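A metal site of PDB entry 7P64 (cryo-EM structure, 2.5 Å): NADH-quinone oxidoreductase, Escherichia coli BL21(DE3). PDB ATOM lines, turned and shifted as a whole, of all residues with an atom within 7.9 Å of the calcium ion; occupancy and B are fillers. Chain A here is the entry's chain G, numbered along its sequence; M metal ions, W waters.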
ATOM      1  N   GLU A 614       5.838 -23.461  -9.219  1.00  0.00           N
ATOM      2  CA  GLU A 614       4.833 -23.373 -10.267  1.00  0.00           C
ATOM      3  C   GLU A 614       5.412 -23.603 -11.659  1.00  0.00           C
ATOM      4  O   GLU A 614       4.771 -23.288 -12.660  1.00  0.00           O
ATOM      5  CB  GLU A 614       4.139 -22.013 -10.207  1.00  0.00           C
ATOM      6  CG  GLU A 614       3.570 -21.672  -8.844  1.00  0.00           C
ATOM      7  CD  GLU A 614       4.249 -20.488  -8.209  1.00  0.00           C
ATOM      8  OE1 GLU A 614       5.141 -19.886  -8.849  1.00  0.00           O
ATOM      9  OE2 GLU A 614       3.892 -20.140  -7.064  1.00  0.00           O
ATOM     10  N   SER A 615       6.617 -24.154 -11.740  1.00  0.00           N
ATOM     11  CA  SER A 615       7.271 -24.341 -13.024  1.00  0.00           C
ATOM     12  C   SER A 615       7.967 -25.692 -13.069  1.00  0.00           C
ATOM     13  O   SER A 615       8.274 -26.294 -12.037  1.00  0.00           O
ATOM     14  CB  SER A 615       8.290 -23.235 -13.309  1.00  0.00           C
ATOM     15  OG  SER A 615       9.373 -23.274 -12.405  1.00  0.00           O
ATOM     16  N   ASP A 616       8.223 -26.157 -14.285  1.00  0.00           N
ATOM     17  CA  ASP A 616       9.080 -27.294 -14.557  1.00  0.00           C
ATOM     18  C   ASP A 616      10.358 -26.799 -15.216  1.00  0.00           C
ATOM     19  O   ASP A 616      10.387 -25.736 -15.834  1.00  0.00           O
ATOM     20  CB  ASP A 616       8.384 -28.299 -15.474  1.00  0.00           C
ATOM     21  CG  ASP A 616       6.924 -28.484 -15.145  1.00  0.00           C
ATOM     22  OD1 ASP A 616       6.620 -29.198 -14.170  1.00  0.00           O
ATOM     23  OD2 ASP A 616       6.087 -27.894 -15.846  1.00  0.00           O
ATOM     24  N   GLY A 617      11.416 -27.581 -15.069  1.00  0.00           N
ATOM     25  CA  GLY A 617      12.658 -27.211 -15.712  1.00  0.00           C
ATOM     26  C   GLY A 617      13.786 -28.123 -15.291  1.00  0.00           C
ATOM     27  O   GLY A 617      13.580 -29.118 -14.603  1.00  0.00           O
ATOM     28  N   PHE A 630       9.748 -30.421 -11.124  1.00  0.00           N
ATOM     29  CA  PHE A 630       8.406 -30.515 -11.660  1.00  0.00           C
ATOM     30  C   PHE A 630       7.506 -29.515 -10.945  1.00  0.00           C
ATOM     31  O   PHE A 630       7.742 -29.153  -9.795  1.00  0.00           O
ATOM     32  CB  PHE A 630       7.857 -31.932 -11.511  1.00  0.00           C
ATOM     33  CG  PHE A 630       8.660 -32.988 -12.226  1.00  0.00           C
ATOM     34  CD1 PHE A 630       9.783 -33.545 -11.631  1.00  0.00           C
ATOM     35  CD2 PHE A 630       8.297 -33.425 -13.479  1.00  0.00           C
ATOM     36  CE1 PHE A 630      10.524 -34.515 -12.286  1.00  0.00           C
ATOM     37  CE2 PHE A 630       9.024 -34.394 -14.131  1.00  0.00           C
ATOM     38  CZ  PHE A 630      10.134 -34.933 -13.538  1.00  0.00           C
ATOM     39  N   GLN A 631       6.469 -29.061 -11.655  1.00  0.00           N
ATOM     40  CA  GLN A 631       5.530 -28.108 -11.088  1.00  0.00           C
ATOM     41  C   GLN A 631       4.733 -28.739  -9.966  1.00  0.00           C
ATOM     42  O   GLN A 631       4.259 -29.870 -10.075  1.00  0.00           O
ATOM     43  CB  GLN A 631       4.599 -27.583 -12.182  1.00  0.00           C
ATOM     44  CG  GLN A 631       3.556 -26.617 -11.714  1.00  0.00           C
ATOM     45  CD  GLN A 631       2.814 -25.961 -12.855  1.00  0.00           C
ATOM     46  OE1 GLN A 631       3.174 -26.124 -14.017  1.00  0.00           O
ATOM     47  NE2 GLN A 631       1.768 -25.226 -12.538  1.00  0.00           N
ATOM     48  N   VAL A 632       4.578 -28.006  -8.865  1.00  0.00           N
ATOM     49  CA  VAL A 632       3.853 -28.538  -7.709  1.00  0.00           C
ATOM     50  C   VAL A 632       2.361 -28.324  -7.860  1.00  0.00           C
ATOM     51  O   VAL A 632       1.567 -29.241  -7.645  1.00  0.00           O
ATOM     52  CB  VAL A 632       4.389 -27.922  -6.412  1.00  0.00           C
ATOM     53  CG1 VAL A 632       3.839 -28.651  -5.206  1.00  0.00           C
ATOM     54  CG2 VAL A 632       5.890 -27.946  -6.398  1.00  0.00           C
ATOM     55  N   TYR A 633       1.959 -27.116  -8.224  1.00  0.00           N
ATOM     56  CA  TYR A 633       0.539 -26.784  -8.277  1.00  0.00           C
ATOM     57  C   TYR A 633       0.272 -25.807  -9.400  1.00  0.00           C
ATOM     58  O   TYR A 633       1.181 -25.142  -9.902  1.00  0.00           O
ATOM     59  CB  TYR A 633       0.048 -26.220  -6.935  1.00  0.00           C
ATOM     60  CG  TYR A 633       0.511 -24.812  -6.653  1.00  0.00           C
ATOM     61  CD1 TYR A 633       1.800 -24.559  -6.192  1.00  0.00           C
ATOM     62  CD2 TYR A 633      -0.336 -23.727  -6.839  1.00  0.00           C
ATOM     63  CE1 TYR A 633       2.222 -23.277  -5.928  1.00  0.00           C
ATOM     64  CE2 TYR A 633       0.076 -22.446  -6.585  1.00  0.00           C
ATOM     65  CZ  TYR A 633       1.363 -22.224  -6.127  1.00  0.00           C
ATOM     66  OH  TYR A 633       1.775 -20.943  -5.873  1.00  0.00           O
ATOM     67  N   ASP A 634      -0.994 -25.734  -9.793  1.00  0.00           N
ATOM     68  CA  ASP A 634      -1.455 -24.753 -10.762  1.00  0.00           C
ATOM     69  C   ASP A 634      -1.776 -23.449 -10.042  1.00  0.00           C
ATOM     70  O   ASP A 634      -2.668 -23.446  -9.183  1.00  0.00           O
ATOM     71  CB  ASP A 634      -2.679 -25.281 -11.492  1.00  0.00           C
ATOM     72  CG  ASP A 634      -3.077 -24.431 -12.686  1.00  0.00           C
ATOM     73  OD1 ASP A 634      -2.305 -23.540 -13.086  1.00  0.00           O
ATOM     74  OD2 ASP A 634      -4.179 -24.661 -13.231  1.00  0.00           O
ATOM     75  N   PRO A 635      -1.091 -22.350 -10.334  1.00  0.00           N
ATOM     76  CA  PRO A 635      -1.417 -21.075  -9.671  1.00  0.00           C
ATOM     77  C   PRO A 635      -2.798 -20.539 -10.013  1.00  0.00           C
ATOM     78  O   PRO A 635      -3.354 -19.766  -9.221  1.00  0.00           O
ATOM     79  CB  PRO A 635      -0.326 -20.115 -10.166  1.00  0.00           C
ATOM     80  CG  PRO A 635       0.658 -20.937 -10.891  1.00  0.00           C
ATOM     81  CD  PRO A 635       0.016 -22.211 -11.295  1.00  0.00           C
ATOM     82  N   LEU A 645       3.126 -17.894 -15.764  1.00  0.00           N
ATOM     83  CA  LEU A 645       3.596 -18.973 -16.627  1.00  0.00           C
ATOM     84  C   LEU A 645       5.066 -19.236 -16.374  1.00  0.00           C
ATOM     85  O   LEU A 645       5.767 -18.457 -15.727  1.00  0.00           O
ATOM     86  CB  LEU A 645       3.359 -18.645 -18.095  1.00  0.00           C
ATOM     87  CG  LEU A 645       1.919 -18.396 -18.526  1.00  0.00           C
ATOM     88  CD1 LEU A 645       1.871 -17.922 -19.967  1.00  0.00           C
ATOM     89  CD2 LEU A 645       1.092 -19.649 -18.349  1.00  0.00           C
ATOM     90  N   GLU A 646       5.536 -20.360 -16.914  1.00  0.00           N
ATOM     91  CA  GLU A 646       6.961 -20.657 -16.890  1.00  0.00           C
ATOM     92  C   GLU A 646       7.710 -19.642 -17.730  1.00  0.00           C
ATOM     93  O   GLU A 646       7.190 -19.105 -18.715  1.00  0.00           O
ATOM     94  CB  GLU A 646       7.214 -22.068 -17.427  1.00  0.00           C
ATOM     95  CG  GLU A 646       6.692 -23.163 -16.537  1.00  0.00           C
ATOM     96  CD  GLU A 646       5.331 -23.655 -16.940  1.00  0.00           C
ATOM     97  OE1 GLU A 646       4.618 -22.936 -17.679  1.00  0.00           O
ATOM     98  OE2 GLU A 646       4.969 -24.778 -16.530  1.00  0.00           O
ATOM     99  N   TRP A 648      10.373 -20.060 -19.627  1.00  0.00           N
ATOM    100  CA  TRP A 648      10.617 -20.545 -20.973  1.00  0.00           C
ATOM    101  C   TRP A 648       9.344 -20.504 -21.813  1.00  0.00           C
ATOM    102  O   TRP A 648       9.423 -20.259 -23.022  1.00  0.00           O
ATOM    103  CB  TRP A 648      11.189 -21.962 -20.962  1.00  0.00           C
ATOM    104  CG  TRP A 648      10.616 -22.901 -19.948  1.00  0.00           C
ATOM    105  CD1 TRP A 648      11.092 -23.141 -18.699  1.00  0.00           C
ATOM    106  CD2 TRP A 648       9.486 -23.760 -20.122  1.00  0.00           C
ATOM    107  NE1 TRP A 648      10.323 -24.075 -18.075  1.00  0.00           N
ATOM    108  CE2 TRP A 648       9.326 -24.470 -18.923  1.00  0.00           C
ATOM    109  CE3 TRP A 648       8.587 -23.987 -21.163  1.00  0.00           C
ATOM    110  CZ2 TRP A 648       8.308 -25.402 -18.736  1.00  0.00           C
ATOM    111  CZ3 TRP A 648       7.578 -24.913 -20.975  1.00  0.00           C
ATOM    112  CH2 TRP A 648       7.442 -25.605 -19.772  1.00  0.00           C
ATOM    113  N   ARG A 649       8.180 -20.718 -21.199  1.00  0.00           N
ATOM    114  CA  ARG A 649       6.925 -20.592 -21.936  1.00  0.00           C
ATOM    115  C   ARG A 649       6.691 -19.147 -22.385  1.00  0.00           C
ATOM    116  O   ARG A 649       6.326 -18.910 -23.542  1.00  0.00           O
ATOM    117  CB  ARG A 649       5.768 -21.082 -21.061  1.00  0.00           C
ATOM    118  CG  ARG A 649       4.428 -21.139 -21.758  1.00  0.00           C
ATOM    119  CD  ARG A 649       3.504 -22.101 -21.067  1.00  0.00           C
ATOM    120  NE  ARG A 649       3.476 -23.391 -21.727  1.00  0.00           N
ATOM    121  CZ  ARG A 649       3.626 -24.561 -21.107  1.00  0.00           C
ATOM    122  NH1 ARG A 649       3.815 -24.632 -19.804  1.00  0.00           N
ATOM    123  NH2 ARG A 649       3.594 -25.680 -21.822  1.00  0.00           N
ATOM    124  N   LEU A 668       7.050 -28.563 -22.801  1.00  0.00           N
ATOM    125  CA  LEU A 668       8.354 -28.573 -22.118  1.00  0.00           C
ATOM    126  C   LEU A 668       9.363 -29.444 -22.847  1.00  0.00           C
ATOM    127  O   LEU A 668      10.522 -29.046 -23.021  1.00  0.00           O
ATOM    128  CB  LEU A 668       8.194 -29.038 -20.674  1.00  0.00           C
ATOM    129  CG  LEU A 668       9.481 -29.412 -19.932  1.00  0.00           C
ATOM    130  CD1 LEU A 668      10.365 -28.190 -19.678  1.00  0.00           C
ATOM    131  CD2 LEU A 668       9.194 -30.127 -18.638  1.00  0.00           C
ATOM    132  N   ARG A 703       0.334 -36.613  -8.072  1.00  0.00           N
ATOM    133  CA  ARG A 703       0.947 -35.569  -7.269  1.00  0.00           C
ATOM    134  C   ARG A 703       0.446 -35.540  -5.837  1.00  0.00           C
ATOM    135  O   ARG A 703       1.120 -34.982  -4.976  1.00  0.00           O
ATOM    136  CB  ARG A 703       0.701 -34.198  -7.905  1.00  0.00           C
ATOM    137  CG  ARG A 703       1.763 -33.759  -8.878  1.00  0.00           C
ATOM    138  CD  ARG A 703       1.544 -32.312  -9.284  1.00  0.00           C
ATOM    139  NE  ARG A 703       2.536 -31.864 -10.253  1.00  0.00           N
ATOM    140  CZ  ARG A 703       2.398 -31.962 -11.563  1.00  0.00           C
ATOM    141  NH1 ARG A 703       1.311 -32.502 -12.097  1.00  0.00           N
ATOM    142  NH2 ARG A 703       3.359 -31.516 -12.351  1.00  0.00           N
ATOM    143  N   GLN A 727      -4.780 -29.486 -16.202  1.00  0.00           N
ATOM    144  CA  GLN A 727      -4.076 -30.404 -17.072  1.00  0.00           C
ATOM    145  C   GLN A 727      -2.585 -30.130 -17.043  1.00  0.00           C
ATOM    146  O   GLN A 727      -2.146 -28.972 -16.982  1.00  0.00           O
ATOM    147  CB  GLN A 727      -4.603 -30.288 -18.502  1.00  0.00           C
ATOM    148  CG  GLN A 727      -6.061 -30.677 -18.656  1.00  0.00           C
ATOM    149  CD  GLN A 727      -6.361 -32.034 -18.052  1.00  0.00           C
ATOM    150  OE1 GLN A 727      -7.121 -32.147 -17.099  1.00  0.00           O
ATOM    151  NE2 GLN A 727      -5.753 -33.069 -18.616  1.00  0.00           N
ATOM    152  N   ASP A 728      -1.785 -31.199 -17.075  1.00  0.00           N
ATOM    153  CA  ASP A 728      -0.336 -31.104 -17.121  1.00  0.00           C
ATOM    154  C   ASP A 728       0.136 -31.681 -18.444  1.00  0.00           C
ATOM    155  O   ASP A 728       0.376 -32.892 -18.555  1.00  0.00           O
ATOM    156  CB  ASP A 728       0.308 -31.823 -15.939  1.00  0.00           C
ATOM    157  CG  ASP A 728       1.769 -31.488 -15.789  1.00  0.00           C
ATOM    158  OD1 ASP A 728       2.223 -30.494 -16.382  1.00  0.00           O
ATOM    159  OD2 ASP A 728       2.482 -32.218 -15.077  1.00  0.00           O
ATOM    160  N   ILE A 729       0.265 -30.824 -19.449  1.00  0.00           N
ATOM    161  CA  ILE A 729       0.806 -31.249 -20.736  1.00  0.00           C
ATOM    162  C   ILE A 729       2.326 -31.299 -20.725  1.00  0.00           C
ATOM    163  O   ILE A 729       2.924 -31.854 -21.658  1.00  0.00           O
ATOM    164  CB  ILE A 729       0.344 -30.327 -21.876  1.00  0.00           C
ATOM    165  CG1 ILE A 729       0.870 -28.904 -21.652  1.00  0.00           C
ATOM    166  CG2 ILE A 729      -1.167 -30.320 -21.973  1.00  0.00           C
ATOM    167  CD1 ILE A 729       1.050 -28.116 -22.930  1.00  0.00           C
ATOM    168  N   ASP A 730       2.973 -30.747 -19.697  1.00  0.00           N
ATOM    169  CA  ASP A 730       4.424 -30.631 -19.700  1.00  0.00           C
ATOM    170  C   ASP A 730       5.099 -31.900 -19.205  1.00  0.00           C
ATOM    171  O   ASP A 730       6.105 -32.332 -19.779  1.00  0.00           O
ATOM    172  CB  ASP A 730       4.857 -29.445 -18.838  1.00  0.00           C
ATOM    173  CG  ASP A 730       4.626 -28.132 -19.525  1.00  0.00           C
ATOM    174  OD1 ASP A 730       4.775 -28.060 -20.758  1.00  0.00           O
ATOM    175  OD2 ASP A 730       4.298 -27.151 -18.828  1.00  0.00           O
ATOM    176  N   THR A 731       4.589 -32.512 -18.141  1.00  0.00           N
ATOM    177  CA  THR A 731       5.271 -33.612 -17.482  1.00  0.00           C
ATOM    178  C   THR A 731       4.382 -34.838 -17.416  1.00  0.00           C
ATOM    179  O   THR A 731       3.213 -34.828 -17.808  1.00  0.00           O
ATOM    180  CB  THR A 731       5.727 -33.221 -16.064  1.00  0.00           C
ATOM    181  OG1 THR A 731       4.589 -33.142 -15.200  1.00  0.00           O
ATOM    182  CG2 THR A 731       6.447 -31.882 -16.076  1.00  0.00           C
ATOM    183  N   PHE A 735      -2.156 -33.502 -11.943  1.00  0.00           N
ATOM    184  CA  PHE A 735      -2.547 -32.620 -10.849  1.00  0.00           C
ATOM    185  C   PHE A 735      -3.732 -33.198 -10.087  1.00  0.00           C
ATOM    186  O   PHE A 735      -4.741 -32.514  -9.898  1.00  0.00           O
ATOM    187  CB  PHE A 735      -2.893 -31.228 -11.371  1.00  0.00           C
ATOM    188  CG  PHE A 735      -1.691 -30.402 -11.723  1.00  0.00           C
ATOM    189  CD1 PHE A 735      -0.842 -29.925 -10.738  1.00  0.00           C
ATOM    190  CD2 PHE A 735      -1.423 -30.079 -13.037  1.00  0.00           C
ATOM    191  CE1 PHE A 735       0.251 -29.161 -11.068  1.00  0.00           C
ATOM    192  CE2 PHE A 735      -0.325 -29.322 -13.372  1.00  0.00           C
ATOM    193  CZ  PHE A 735       0.509 -28.858 -12.389  1.00  0.00           C
HETATM  194 CA    CA M   1       3.812 -26.916 -16.328  1.00  0.00          CA
HETATM  195  O   HOH W   1       1.649 -24.772 -16.651  1.00  0.00           O
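The side-chain carboxylate (OE1) of Glu 646 lies within salt-bridge range of the guanidinium group (NH1) of Arg 649, at 2.8 Å. The backbone carbonyl oxygen (O) of Asp 616 is in hydrogen-bond range of the indole nitrogen (NE1) of Trp 648, at 2.8 Å. The backbone NH (N) of Gln 631 is in hydrogen-bond range of the backbone carbonyl oxygen (O) of Ser 615 (3.3 Å). The side-chain amide nitrogen of Gln 631 lies within hydrogen-bond range of the backbone carbonyl oxygen of Tyr 633 (2.7 Å). N of Asp 730 lies close to OD1 of Asp 728 (3.4 Å). OD1 of Asp 730 lies within salt-bridge range of NH2 of Arg 649, 2.9 Å away. OD1 of Asp 730 lies within hydrogen-bond range of N of Leu 668, at 3.1 Å. The side-chain carboxylate (OD2) of Asp 728 lies within salt-bridge range of the guanidinium group (NH2) of Arg 703.
Asp 728 touches the calcium ion (OD1 to CA, 3.9 Å).
The calcium ion is bound by OE2 of Glu 646 (2.4 Å), OD2 of Asp 616 (2.5 Å), OE1 of Gln 631 (2.5 Å) and OD2 of Asp 730 (2.6 Å). Slightly farther from the calcium ion lies water W1 (3.1 Å).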
